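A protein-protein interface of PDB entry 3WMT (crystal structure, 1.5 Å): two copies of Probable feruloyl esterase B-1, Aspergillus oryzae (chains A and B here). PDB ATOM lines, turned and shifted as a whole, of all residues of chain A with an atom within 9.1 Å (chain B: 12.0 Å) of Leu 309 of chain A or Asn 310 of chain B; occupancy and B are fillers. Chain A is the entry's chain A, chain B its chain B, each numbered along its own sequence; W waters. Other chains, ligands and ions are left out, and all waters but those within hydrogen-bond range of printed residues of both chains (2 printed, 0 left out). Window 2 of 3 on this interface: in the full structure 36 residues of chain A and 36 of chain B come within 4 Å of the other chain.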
ATOM      1  N   ASN A 216      36.758  -8.019   8.358  1.00  0.00           N
ATOM      2  CA  ASN A 216      36.638  -7.755   6.917  1.00  0.00           C
ATOM      3  C   ASN A 216      37.641  -8.535   6.050  1.00  0.00           C
ATOM      4  O   ASN A 216      37.324  -8.979   4.939  1.00  0.00           O
ATOM      5  CB  ASN A 216      36.760  -6.279   6.638  1.00  0.00           C
ATOM      6  CG  ASN A 216      35.595  -5.496   7.108  1.00  0.00           C
ATOM      7  OD1 ASN A 216      34.571  -6.008   7.068  1.00  0.00           O
ATOM      8  ND2 ASN A 216      35.689  -4.321   7.392  1.00  0.00           N
ATOM      9  N   THR A 306      36.494  -4.241  -1.903  1.00  0.00           N
ATOM     10  CA  THR A 306      35.167  -4.737  -1.453  1.00  0.00           C
ATOM     11  C   THR A 306      34.533  -3.673  -0.613  1.00  0.00           C
ATOM     12  O   THR A 306      35.117  -3.156   0.333  1.00  0.00           O
ATOM     13  CB  THR A 306      35.398  -5.955  -0.604  1.00  0.00           C
ATOM     14  OG1 THR A 306      35.987  -7.015  -1.348  1.00  0.00           O
ATOM     15  CG2 THR A 306      33.929  -6.553  -0.107  1.00  0.00           C
ATOM     16  N   TYR A 307      33.297  -3.281  -0.911  1.00  0.00           N
ATOM     17  CA  TYR A 307      32.503  -2.323  -0.178  1.00  0.00           C
ATOM     18  C   TYR A 307      31.222  -2.996   0.283  1.00  0.00           C
ATOM     19  O   TYR A 307      30.822  -4.004  -0.312  1.00  0.00           O
ATOM     20  CB  TYR A 307      32.199  -1.090  -1.133  1.00  0.00           C
ATOM     21  CG  TYR A 307      33.321  -0.043  -1.208  1.00  0.00           C
ATOM     22  CD1 TYR A 307      34.509  -0.325  -1.867  1.00  0.00           C
ATOM     23  CD2 TYR A 307      33.274   1.102  -0.463  1.00  0.00           C
ATOM     24  CE1 TYR A 307      35.539   0.640  -1.848  1.00  0.00           C
ATOM     25  CE2 TYR A 307      34.270   2.076  -0.424  1.00  0.00           C
ATOM     26  CZ  TYR A 307      35.418   1.841  -1.112  1.00  0.00           C
ATOM     27  OH  TYR A 307      36.486   2.802  -1.045  1.00  0.00           O
ATOM     28  N   GLY A 308      30.685  -2.387   1.311  1.00  0.00           N
ATOM     29  CA  GLY A 308      29.514  -2.994   1.955  1.00  0.00           C
ATOM     30  C   GLY A 308      28.237  -2.223   1.872  1.00  0.00           C
ATOM     31  O   GLY A 308      28.054  -1.273   1.087  1.00  0.00           O
ATOM     32  N   LEU A 309      27.374  -2.531   2.849  1.00  0.00           N
ATOM     33  CA  LEU A 309      26.122  -1.655   2.942  1.00  0.00           C
ATOM     34  C   LEU A 309      26.444  -0.208   3.230  1.00  0.00           C
ATOM     35  O   LEU A 309      27.473   0.156   3.945  1.00  0.00           O
ATOM     36  CB  LEU A 309      25.299  -2.216   4.155  1.00  0.00           C
ATOM     37  CG  LEU A 309      24.935  -3.678   4.075  1.00  0.00           C
ATOM     38  CD1 LEU A 309      24.007  -3.985   5.333  1.00  0.00           C
ATOM     39  CD2 LEU A 309      24.178  -4.004   2.818  1.00  0.00           C
ATOM     40  N   ASN A 310      25.617   0.739   2.767  1.00  0.00           N
ATOM     41  CA  ASN A 310      25.807   2.151   2.965  1.00  0.00           C
ATOM     42  C   ASN A 310      27.037   2.651   2.189  1.00  0.00           C
ATOM     43  O   ASN A 310      27.584   3.673   2.590  1.00  0.00           O
ATOM     44  CB  ASN A 310      25.848   2.539   4.470  1.00  0.00           C
ATOM     45  CG  ASN A 310      25.712   4.075   4.756  1.00  0.00           C
ATOM     46  OD1 ASN A 310      24.891   4.760   4.124  1.00  0.00           O
ATOM     47  ND2 ASN A 310      26.538   4.614   5.740  1.00  0.00           N
ATOM     48  N   GLY A 311      27.549   1.723   1.328  1.00  0.00           N
ATOM     49  CA  GLY A 311      28.726   2.008   0.440  1.00  0.00           C
ATOM     50  C   GLY A 311      30.055   2.170   1.193  1.00  0.00           C
ATOM     51  O   GLY A 311      30.902   3.002   0.815  1.00  0.00           O
ATOM     52  N   SER A 312      30.197   1.535   2.324  1.00  0.00           N
ATOM     53  CA  SER A 312      31.355   1.717   3.174  1.00  0.00           C
ATOM     54  C   SER A 312      32.500   0.733   2.750  1.00  0.00           C
ATOM     55  O   SER A 312      32.243  -0.372   2.335  1.00  0.00           O
ATOM     56  CB  SER A 312      30.993   1.405   4.625  1.00  0.00           C
ATOM     57  OG  SER A 312      30.248   0.199   4.683  1.00  0.00           O
ATOM     58  N   PHE A 313      33.690   1.280   2.757  1.00  0.00           N
ATOM     59  CA  PHE A 313      34.869   0.427   2.495  1.00  0.00           C
ATOM     60  C   PHE A 313      34.951  -0.729   3.478  1.00  0.00           C
ATOM     61  O   PHE A 313      34.869  -0.535   4.656  1.00  0.00           O
ATOM     62  CB  PHE A 313      36.109   1.310   2.680  1.00  0.00           C
ATOM     63  CG  PHE A 313      37.438   0.595   2.302  1.00  0.00           C
ATOM     64  CD1 PHE A 313      37.910   0.619   1.040  1.00  0.00           C
ATOM     65  CD2 PHE A 313      38.151  -0.028   3.290  1.00  0.00           C
ATOM     66  CE1 PHE A 313      39.170   0.036   0.708  1.00  0.00           C
ATOM     67  CE2 PHE A 313      39.431  -0.637   2.973  1.00  0.00           C
ATOM     68  CZ  PHE A 313      39.875  -0.600   1.689  1.00  0.00           C
ATOM     69  N   LEU A 314      35.193  -1.935   2.956  1.00  0.00           N
ATOM     70  CA  LEU A 314      35.305  -3.155   3.745  1.00  0.00           C
ATOM     71  C   LEU A 314      36.784  -3.669   3.719  1.00  0.00           C
ATOM     72  O   LEU A 314      37.374  -3.792   4.726  1.00  0.00           O
ATOM     73  CB  LEU A 314      34.412  -4.210   3.190  1.00  0.00           C
ATOM     74  CG  LEU A 314      33.330  -4.768   4.028  1.00  0.00           C
ATOM     75  CD1 LEU A 314      32.693  -3.466   4.538  1.00  0.00           C
ATOM     76  CD2 LEU A 314      32.226  -5.600   3.466  1.00  0.00           C
ATOM     77  N   TRP A 358      27.645 -16.196   1.063  1.00  0.00           N
ATOM     78  CA  TRP A 358      28.100 -14.979   1.648  1.00  0.00           C
ATOM     79  C   TRP A 358      27.679 -13.765   0.923  1.00  0.00           C
ATOM     80  O   TRP A 358      27.745 -13.771  -0.338  1.00  0.00           O
ATOM     81  CB  TRP A 358      29.680 -14.928   1.699  1.00  0.00           C
ATOM     82  CG  TRP A 358      30.240 -13.664   2.279  1.00  0.00           C
ATOM     83  CD1 TRP A 358      30.470 -13.394   3.625  1.00  0.00           C
ATOM     84  CD2 TRP A 358      30.600 -12.506   1.575  1.00  0.00           C
ATOM     85  NE1 TRP A 358      30.927 -12.134   3.733  1.00  0.00           N
ATOM     86  CE2 TRP A 358      31.001 -11.539   2.484  1.00  0.00           C
ATOM     87  CE3 TRP A 358      30.585 -12.169   0.218  1.00  0.00           C
ATOM     88  CZ2 TRP A 358      31.393 -10.261   2.098  1.00  0.00           C
ATOM     89  CZ3 TRP A 358      30.924 -10.908  -0.149  1.00  0.00           C
ATOM     90  CH2 TRP A 358      31.353  -9.983   0.751  1.00  0.00           C
ATOM     91  N   THR A 359      27.191 -12.748   1.608  1.00  0.00           N
ATOM     92  CA  THR A 359      26.857 -11.495   1.124  1.00  0.00           C
ATOM     93  C   THR A 359      27.404 -10.367   1.977  1.00  0.00           C
ATOM     94  O   THR A 359      27.849 -10.544   3.160  1.00  0.00           O
ATOM     95  CB  THR A 359      25.321 -11.264   1.161  1.00  0.00           C
ATOM     96  OG1 THR A 359      24.935 -11.318   2.547  1.00  0.00           O
ATOM     97  CG2 THR A 359      24.602 -12.337   0.369  1.00  0.00           C
ATOM     98  N   VAL A 360      27.389  -9.145   1.473  1.00  0.00           N
ATOM     99  CA  VAL A 360      27.768  -7.980   2.279  1.00  0.00           C
ATOM    100  C   VAL A 360      26.843  -7.780   3.481  1.00  0.00           C
ATOM    101  O   VAL A 360      27.283  -7.190   4.471  1.00  0.00           O
ATOM    102  CB  VAL A 360      27.890  -6.650   1.489  1.00  0.00           C
ATOM    103  CG1 VAL A 360      29.009  -6.786   0.496  1.00  0.00           C
ATOM    104  CG2 VAL A 360      26.632  -6.304   0.766  1.00  0.00           C
ATOM    105  N   GLN A 361      25.593  -8.239   3.439  1.00  0.00           N
ATOM    106  CA  GLN A 361      24.750  -8.133   4.604  1.00  0.00           C
ATOM    107  C   GLN A 361      25.302  -9.049   5.704  1.00  0.00           C
ATOM    108  O   GLN A 361      25.348  -8.638   6.874  1.00  0.00           O
ATOM    109  CB  GLN A 361      23.293  -8.530   4.265  1.00  0.00           C
ATOM    110  CG  GLN A 361      22.427  -8.629   5.544  1.00  0.00           C
ATOM    111  CD  GLN A 361      22.172  -7.340   6.381  1.00  0.00           C
ATOM    112  OE1 GLN A 361      22.876  -6.972   7.468  1.00  0.00           O
ATOM    113  NE2 GLN A 361      21.089  -6.656   5.967  1.00  0.00           N
ATOM    114  N   ASP A 362      25.821 -10.204   5.339  1.00  0.00           N
ATOM    115  CA  ASP A 362      26.491 -11.104   6.313  1.00  0.00           C
ATOM    116  C   ASP A 362      27.692 -10.428   6.902  1.00  0.00           C
ATOM    117  O   ASP A 362      27.928 -10.463   8.133  1.00  0.00           O
ATOM    118  CB  ASP A 362      26.924 -12.409   5.684  1.00  0.00           C
ATOM    119  CG  ASP A 362      25.783 -13.224   5.175  1.00  0.00           C
ATOM    120  OD1 ASP A 362      24.642 -13.068   5.642  1.00  0.00           O
ATOM    121  OD2 ASP A 362      26.024 -14.109   4.284  1.00  0.00           O
ATOM    122  N   ALA A 363      28.468  -9.694   6.085  1.00  0.00           N
ATOM    123  CA  ALA A 363      29.647  -9.014   6.574  1.00  0.00           C
ATOM    124  C   ALA A 363      29.279  -7.884   7.522  1.00  0.00           C
ATOM    125  O   ALA A 363      30.002  -7.570   8.476  1.00  0.00           O
ATOM    126  CB  ALA A 363      30.400  -8.501   5.384  1.00  0.00           C
ATOM    127  N   ALA A 364      28.174  -7.211   7.307  1.00  0.00           N
ATOM    128  CA  ALA A 364      27.699  -6.137   8.182  1.00  0.00           C
ATOM    129  C   ALA A 364      27.378  -6.715   9.598  1.00  0.00           C
ATOM    130  O   ALA A 364      27.701  -6.116  10.599  1.00  0.00           O
ATOM    131  CB  ALA A 364      26.465  -5.412   7.650  1.00  0.00           C
ATOM    132  N   ILE A 365      26.746  -7.862   9.607  1.00  0.00           N
ATOM    133  CA  ILE A 365      26.441  -8.558  10.901  1.00  0.00           C
ATOM    134  C   ILE A 365      27.732  -8.845  11.643  1.00  0.00           C
ATOM    135  O   ILE A 365      27.892  -8.513  12.808  1.00  0.00           O
ATOM    136  CB  ILE A 365      25.708  -9.829  10.639  1.00  0.00           C
ATOM    137  CG1 ILE A 365      24.299  -9.573  10.055  1.00  0.00           C
ATOM    138  CG2 ILE A 365      25.549 -10.599  11.921  1.00  0.00           C
ATOM    139  CD1 ILE A 365      23.702 -10.842   9.483  1.00  0.00           C
ATOM    140  N   ALA A 366      28.659  -9.394  10.907  1.00  0.00           N
ATOM    141  CA  ALA A 366      29.972  -9.801  11.486  1.00  0.00           C
ATOM    142  C   ALA A 366      30.690  -8.612  12.010  1.00  0.00           C
ATOM    143  O   ALA A 366      31.352  -8.671  13.094  1.00  0.00           O
ATOM    144  CB  ALA A 366      30.776 -10.608  10.505  1.00  0.00           C
ATOM    145  N   ASN A 367      30.688  -7.507  11.273  1.00  0.00           N
ATOM    146  CA  ASN A 367      31.394  -6.299  11.694  1.00  0.00           C
ATOM    147  C   ASN A 367      30.831  -5.675  12.942  1.00  0.00           C
ATOM    148  O   ASN A 367      31.553  -5.206  13.819  1.00  0.00           O
ATOM    149  CB  ASN A 367      31.448  -5.256  10.572  1.00  0.00           C
ATOM    150  CG  ASN A 367      32.328  -4.078  10.908  1.00  0.00           C
ATOM    151  OD1 ASN A 367      33.534  -4.244  10.965  1.00  0.00           O
ATOM    152  ND2 ASN A 367      31.773  -2.918  11.119  1.00  0.00           N
ATOM    153  N   ALA B 305      36.795   5.748  -5.289  1.00  0.00           N
ATOM    154  CA  ALA B 305      35.598   5.402  -5.951  1.00  0.00           C
ATOM    155  C   ALA B 305      34.384   5.549  -4.994  1.00  0.00           C
ATOM    156  O   ALA B 305      34.570   5.396  -3.747  1.00  0.00           O
ATOM    157  CB  ALA B 305      35.691   4.015  -6.533  1.00  0.00           C
ATOM    158  N   THR B 306      33.221   5.823  -5.550  1.00  0.00           N
ATOM    159  CA  THR B 306      31.954   5.949  -4.842  1.00  0.00           C
ATOM    160  C   THR B 306      31.236   4.649  -5.055  1.00  0.00           C
ATOM    161  O   THR B 306      31.031   4.165  -6.174  1.00  0.00           O
ATOM    162  CB  THR B 306      31.189   7.097  -5.402  1.00  0.00           C
ATOM    163  OG1 THR B 306      31.866   8.324  -5.279  1.00  0.00           O
ATOM    164  CG2 THR B 306      29.805   7.255  -4.690  1.00  0.00           C
ATOM    165  N   TYR B 307      30.777   4.053  -3.949  1.00  0.00           N
ATOM    166  CA  TYR B 307      29.956   2.842  -3.894  1.00  0.00           C
ATOM    167  C   TYR B 307      28.589   3.126  -3.263  1.00  0.00           C
ATOM    168  O   TYR B 307      28.507   4.041  -2.513  1.00  0.00           O
ATOM    169  CB  TYR B 307      30.714   1.746  -3.175  1.00  0.00           C
ATOM    170  CG  TYR B 307      31.865   1.228  -3.954  1.00  0.00           C
ATOM    171  CD1 TYR B 307      31.783   0.071  -4.633  1.00  0.00           C
ATOM    172  CD2 TYR B 307      33.051   1.973  -3.885  1.00  0.00           C
ATOM    173  CE1 TYR B 307      32.954  -0.419  -5.334  1.00  0.00           C
ATOM    174  CE2 TYR B 307      34.161   1.533  -4.534  1.00  0.00           C
ATOM    175  CZ  TYR B 307      34.057   0.425  -5.304  1.00  0.00           C
ATOM    176  OH  TYR B 307      35.405   0.213  -5.755  1.00  0.00           O
ATOM    177  N   GLY B 308      27.648   2.294  -3.609  1.00  0.00           N
ATOM    178  CA  GLY B 308      26.251   2.561  -3.227  1.00  0.00           C
ATOM    179  C   GLY B 308      25.748   1.590  -2.154  1.00  0.00           C
ATOM    180  O   GLY B 308      26.477   0.864  -1.502  1.00  0.00           O
ATOM    181  N   LEU B 309      24.438   1.483  -2.082  1.00  0.00           N
ATOM    182  CA  LEU B 309      23.844   0.324  -1.369  1.00  0.00           C
ATOM    183  C   LEU B 309      24.214  -0.996  -1.952  1.00  0.00           C
ATOM    184  O   LEU B 309      24.421  -1.251  -3.243  1.00  0.00           O
ATOM    185  CB  LEU B 309      22.335   0.447  -1.553  1.00  0.00           C
ATOM    186  CG  LEU B 309      21.792   1.755  -1.020  1.00  0.00           C
ATOM    187  CD1 LEU B 309      20.205   1.715  -1.057  1.00  0.00           C
ATOM    188  CD2 LEU B 309      22.240   2.178   0.354  1.00  0.00           C
ATOM    189  N   ASN B 310      24.325  -1.946  -1.045  1.00  0.00           N
ATOM    190  CA  ASN B 310      24.670  -3.248  -1.300  1.00  0.00           C
ATOM    191  C   ASN B 310      26.105  -3.369  -1.766  1.00  0.00           C
ATOM    192  O   ASN B 310      26.384  -4.346  -2.415  1.00  0.00           O
ATOM    193  CB  ASN B 310      23.625  -3.959  -2.177  1.00  0.00           C
ATOM    194  CG  ASN B 310      22.262  -4.084  -1.471  1.00  0.00           C
ATOM    195  OD1 ASN B 310      22.178  -4.009  -0.236  1.00  0.00           O
ATOM    196  ND2 ASN B 310      21.193  -4.288  -2.244  1.00  0.00           N
ATOM    197  N   GLY B 311      26.822  -2.257  -1.623  1.00  0.00           N
ATOM    198  CA  GLY B 311      28.246  -2.192  -2.008  1.00  0.00           C
ATOM    199  C   GLY B 311      28.554  -2.182  -3.513  1.00  0.00           C
ATOM    200  O   GLY B 311      29.606  -2.629  -3.937  1.00  0.00           O
ATOM    201  N   SER B 312      27.615  -1.729  -4.303  1.00  0.00           N
ATOM    202  CA  SER B 312      27.755  -1.657  -5.760  1.00  0.00           C
ATOM    203  C   SER B 312      28.552  -0.429  -6.165  1.00  0.00           C
ATOM    204  O   SER B 312      28.464   0.617  -5.586  1.00  0.00           O
ATOM    205  CB  SER B 312      26.384  -1.437  -6.387  1.00  0.00           C
ATOM    206  OG  SER B 312      25.771  -2.669  -6.292  1.00  0.00           O
ATOM    207  N   PHE B 313      29.351  -0.657  -7.182  1.00  0.00           N
ATOM    208  CA  PHE B 313      30.194   0.418  -7.802  1.00  0.00           C
ATOM    209  C   PHE B 313      29.230   1.461  -8.380  1.00  0.00           C
ATOM    210  O   PHE B 313      28.265   1.145  -9.057  1.00  0.00           O
ATOM    211  CB  PHE B 313      31.124  -0.125  -8.856  1.00  0.00           C
ATOM    212  CG  PHE B 313      32.020   0.931  -9.527  1.00  0.00           C
ATOM    213  CD1 PHE B 313      33.263   1.192  -9.024  1.00  0.00           C
ATOM    214  CD2 PHE B 313      31.602   1.574 -10.628  1.00  0.00           C
ATOM    215  CE1 PHE B 313      34.132   2.053  -9.648  1.00  0.00           C
ATOM    216  CE2 PHE B 313      32.455   2.479 -11.247  1.00  0.00           C
ATOM    217  CZ  PHE B 313      33.693   2.668 -10.775  1.00  0.00           C
ATOM    218  N   LEU B 314      29.411   2.738  -8.020  1.00  0.00           N
ATOM    219  CA  LEU B 314      28.601   3.835  -8.499  1.00  0.00           C
ATOM    220  C   LEU B 314      29.401   4.665  -9.531  1.00  0.00           C
ATOM    221  O   LEU B 314      28.953   4.907 -10.621  1.00  0.00           O
ATOM    222  CB  LEU B 314      28.206   4.629  -7.281  1.00  0.00           C
ATOM    223  CG  LEU B 314      27.049   5.475  -7.277  1.00  0.00           C
ATOM    224  CD1 LEU B 314      26.306   5.427  -5.943  1.00  0.00           C
ATOM    225  CD2 LEU B 314      27.562   6.915  -7.587  1.00  0.00           C
ATOM    226  N   TRP B 358      22.698  14.952   0.403  1.00  0.00           N
ATOM    227  CA  TRP B 358      22.798  13.758  -0.466  1.00  0.00           C
ATOM    228  C   TRP B 358      23.368  12.536   0.235  1.00  0.00           C
ATOM    229  O   TRP B 358      24.370  12.650   0.966  1.00  0.00           O
ATOM    230  CB  TRP B 358      23.698  14.078  -1.732  1.00  0.00           C
ATOM    231  CG  TRP B 358      23.957  12.934  -2.608  1.00  0.00           C
ATOM    232  CD1 TRP B 358      23.188  12.561  -3.641  1.00  0.00           C
ATOM    233  CD2 TRP B 358      25.012  11.968  -2.538  1.00  0.00           C
ATOM    234  NE1 TRP B 358      23.648  11.441  -4.212  1.00  0.00           N
ATOM    235  CE2 TRP B 358      24.789  11.012  -3.561  1.00  0.00           C
ATOM    236  CE3 TRP B 358      26.085  11.794  -1.676  1.00  0.00           C
ATOM    237  CZ2 TRP B 358      25.616   9.885  -3.742  1.00  0.00           C
ATOM    238  CZ3 TRP B 358      26.875  10.746  -1.846  1.00  0.00           C
ATOM    239  CH2 TRP B 358      26.687   9.790  -2.891  1.00  0.00           C
ATOM    240  N   THR B 359      22.786  11.370  -0.067  1.00  0.00           N
ATOM    241  CA  THR B 359      23.216  10.108   0.406  1.00  0.00           C
ATOM    242  C   THR B 359      23.157   9.075  -0.684  1.00  0.00           C
ATOM    243  O   THR B 359      22.530   9.266  -1.745  1.00  0.00           O
ATOM    244  CB  THR B 359      22.297   9.581   1.538  1.00  0.00           C
ATOM    245  OG1 THR B 359      21.023   9.343   0.977  1.00  0.00           O
ATOM    246  CG2 THR B 359      22.190  10.590   2.658  1.00  0.00           C
ATOM    247  N   VAL B 360      23.799   7.942  -0.475  1.00  0.00           N
ATOM    248  CA  VAL B 360      23.716   6.850  -1.396  1.00  0.00           C
ATOM    249  C   VAL B 360      22.296   6.303  -1.545  1.00  0.00           C
ATOM    250  O   VAL B 360      21.955   5.786  -2.565  1.00  0.00           O
ATOM    251  CB  VAL B 360      24.678   5.683  -1.108  1.00  0.00           C
ATOM    252  CG1 VAL B 360      26.100   6.203  -1.363  1.00  0.00           C
ATOM    253  CG2 VAL B 360      24.477   5.120   0.293  1.00  0.00           C
ATOM    254  N   GLN B 361      21.469   6.433  -0.547  1.00  0.00           N
ATOM    255  CA  GLN B 361      20.044   6.131  -0.693  1.00  0.00           C
ATOM    256  C   GLN B 361      19.383   6.978  -1.770  1.00  0.00           C
ATOM    257  O   GLN B 361      18.690   6.474  -2.625  1.00  0.00           O
ATOM    258  CB  GLN B 361      19.330   6.318   0.663  1.00  0.00           C
ATOM    259  CG  GLN B 361      17.849   5.944   0.514  1.00  0.00           C
ATOM    260  CD  GLN B 361      16.910   6.151   1.713  1.00  0.00           C
ATOM    261  OE1 GLN B 361      17.311   6.399   2.857  1.00  0.00           O
ATOM    262  NE2 GLN B 361      15.635   6.039   1.427  1.00  0.00           N
ATOM    263  N   ASP B 362      19.692   8.252  -1.759  1.00  0.00           N
ATOM    264  CA  ASP B 362      19.225   9.187  -2.825  1.00  0.00           C
ATOM    265  C   ASP B 362      19.705   8.686  -4.181  1.00  0.00           C
ATOM    266  O   ASP B 362      19.001   8.696  -5.207  1.00  0.00           O
ATOM    267  CB  ASP B 362      19.705  10.602  -2.616  1.00  0.00           C
ATOM    268  CG  ASP B 362      19.240  11.156  -1.322  1.00  0.00           C
ATOM    269  OD1 ASP B 362      18.107  10.774  -0.865  1.00  0.00           O
ATOM    270  OD2 ASP B 362      19.837  12.032  -0.762  1.00  0.00           O
ATOM    271  N   ALA B 363      20.990   8.278  -4.258  1.00  0.00           N
ATOM    272  CA  ALA B 363      21.519   7.852  -5.528  1.00  0.00           C
ATOM    273  C   ALA B 363      20.813   6.620  -6.051  1.00  0.00           C
ATOM    274  O   ALA B 363      20.665   6.443  -7.225  1.00  0.00           O
ATOM    275  CB  ALA B 363      23.046   7.573  -5.373  1.00  0.00           C
ATOM    276  N   ALA B 364      20.441   5.696  -5.137  1.00  0.00           N
ATOM    277  CA  ALA B 364      19.759   4.502  -5.509  1.00  0.00           C
ATOM    278  C   ALA B 364      18.357   4.838  -6.104  1.00  0.00           C
ATOM    279  O   ALA B 364      17.955   4.212  -7.068  1.00  0.00           O
ATOM    280  CB  ALA B 364      19.606   3.556  -4.307  1.00  0.00           C
ATOM    281  N   ILE B 365      17.665   5.781  -5.493  1.00  0.00           N
ATOM    282  CA  ILE B 365      16.369   6.286  -6.033  1.00  0.00           C
ATOM    283  C   ILE B 365      16.608   6.838  -7.436  1.00  0.00           C
ATOM    284  O   ILE B 365      15.864   6.540  -8.378  1.00  0.00           O
ATOM    285  CB  ILE B 365      15.769   7.285  -5.112  1.00  0.00           C
ATOM    286  CG1 ILE B 365      15.423   6.539  -3.767  1.00  0.00           C
ATOM    287  CG2 ILE B 365      14.541   7.921  -5.741  1.00  0.00           C
ATOM    288  CD1 ILE B 365      14.971   7.436  -2.660  1.00  0.00           C
ATOM    289  N   ASN B 367      19.014   6.207  -9.605  1.00  0.00           N
ATOM    290  CA  ASN B 367      19.370   5.143 -10.488  1.00  0.00           C
ATOM    291  C   ASN B 367      18.156   4.301 -10.942  1.00  0.00           C
ATOM    292  O   ASN B 367      18.101   3.850 -12.108  1.00  0.00           O
ATOM    293  CB  ASN B 367      20.415   4.181  -9.839  1.00  0.00           C
ATOM    294  CG  ASN B 367      21.016   3.195 -10.801  1.00  0.00           C
ATOM    295  OD1 ASN B 367      21.634   3.556 -11.790  1.00  0.00           O
ATOM    296  ND2 ASN B 367      20.830   1.909 -10.523  1.00  0.00           N
ATOM    297  N   ALA B 368      17.269   4.013  -9.985  1.00  0.00           N
ATOM    298  CA  ALA B 368      16.077   3.227 -10.305  1.00  0.00           C
ATOM    299  C   ALA B 368      15.231   3.945 -11.315  1.00  0.00           C
ATOM    300  O   ALA B 368      14.633   3.280 -12.203  1.00  0.00           O
ATOM    301  CB  ALA B 368      15.274   2.855  -9.075  1.00  0.00           C
HETATM  302  O   HOH W   1      31.510   4.875  -1.171  1.00  0.00           O
HETATM  303  O   HOH W   2      31.891  -4.130  -3.378  1.00  0.00           O
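The backbone carbonyl oxygen (O) of Gly 308 of chain A sits at hydrogen-bond distance from the backbone NH (N) of Gly 311 of chain B (3.1 Å). The backbone NH of Gly 311 of chain A lies within hydrogen-bond range of the backbone carbonyl oxygen of Gly 308 of chain B (3.1 Å).
The side-chain hydroxyl (OG) of Ser 312 of chain A lies within hydrogen-bond range of the backbone carbonyl oxygen (O) of Leu 309 of chain A (2.9 Å).
Among the printed residues, merely in contact across the chains: Tyr 307 of chain A with Tyr 307 of chain B (3.1 Å), Tyr 307 of chain A with Gly 311 of chain B (3.6 Å), Gly 311 of chain A with Tyr 307 of chain B (3.6 Å), Leu 309 of chain A with Asn 310 of chain B (3.7 Å), Gly 308 of chain A with Gly 308 of chain B (3.7 Å), Val 360 of chain A with Asn 310 of chain B (3.7 Å) and Asn 310 of chain A with Val 360 of chain B (3.9 Å).
Of chain B, only Asn 310 (3.7 Å) comes within 4 Å of Leu 309 of chain A. Of chain A, only Leu 309 and Val 360 come within 4 Å of Asn 310 of chain B. Of chain B, only Gly 308 and Gly 311 come within 4 Å of Gly 308 of chain A. Asn 310 of chain A touches just one residue of chain B: Val 360 (3.9 Å). No residue of chain B comes within 4 Å of Ser 312 of chain A. Of chain B, only Asn 310 (3.7 Å) comes within 4 Å of Val 360 of chain A. No residue of chain B comes within 4 Å of Gln 361 of chain A. No residue of chain B comes within 4 Å of Ala 363 of chain A. No residue of chain B comes within 4 Å of Ala 364 of chain A. Of the printed residues of chain B, Tyr 307 of chain A touches Tyr 307 (3.1 Å) and Gly 311 (3.6 Å). Of the printed residues of chain A, Gly 308 of chain B touches Gly 308 and Gly 311. Printed residues of chain A within 4 Å of Val 360 of chain B: Asn 310. Thr 306 of chain B touches none of the printed residues of chain A. The nearest residue of chain B that does not touch Leu 309 of chain A is Gly 311 of chain B (4.5 Å).
Printed residues of chain A that touch a printed residue of chain B: Tyr 307, Gly 308, Leu 309, Asn 310, Gly 311 and Val 360. Hydrophobic or aromatic side chains of chain A within 4 Å of the printed part of chain B: Tyr 307, Leu 309 and Val 360. Of the 20 printed residues of chain B, 5 touch a printed residue of chain A. Hydrophobic or aromatic side chains of chain B within 4 Å of the printed part of chain A: Tyr 307 and Val 360. Among the printed residues, no Asp or Glu carboxylate lies within 4 Å of a Lys or Arg side-chain nitrogen of the other chain.
Tyr 307 of chain A touches its own counterpart, Tyr 307 of chain B. Tyr 307 of chain A touches Gly 311 of chain B, and with the chains exchanged Gly 311 of chain A touches Tyr 307 of chain B. Gly 308 of chain A touches Gly 311 of chain B, and with the chains exchanged Gly 311 of chain A touches Gly 308 of chain B. Leu 309 of chain A touches Asn 310 of chain B, but with the chains exchanged Asn 310 of chain A does not touch Leu 309 of chain B (4.4 Å).
Water W2 lies within hydrogen-bond range of the backbone carbonyl oxygen (O) of Gly 311 of chain B (2.8 Å) and the backbone NH (N) of Tyr 307 of chain A (3.0 Å). Water W1 lies within hydrogen-bond range of O of Gly 311 of chain A (2.8 Å) and N of Tyr 307 of chain B (3.0 Å).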
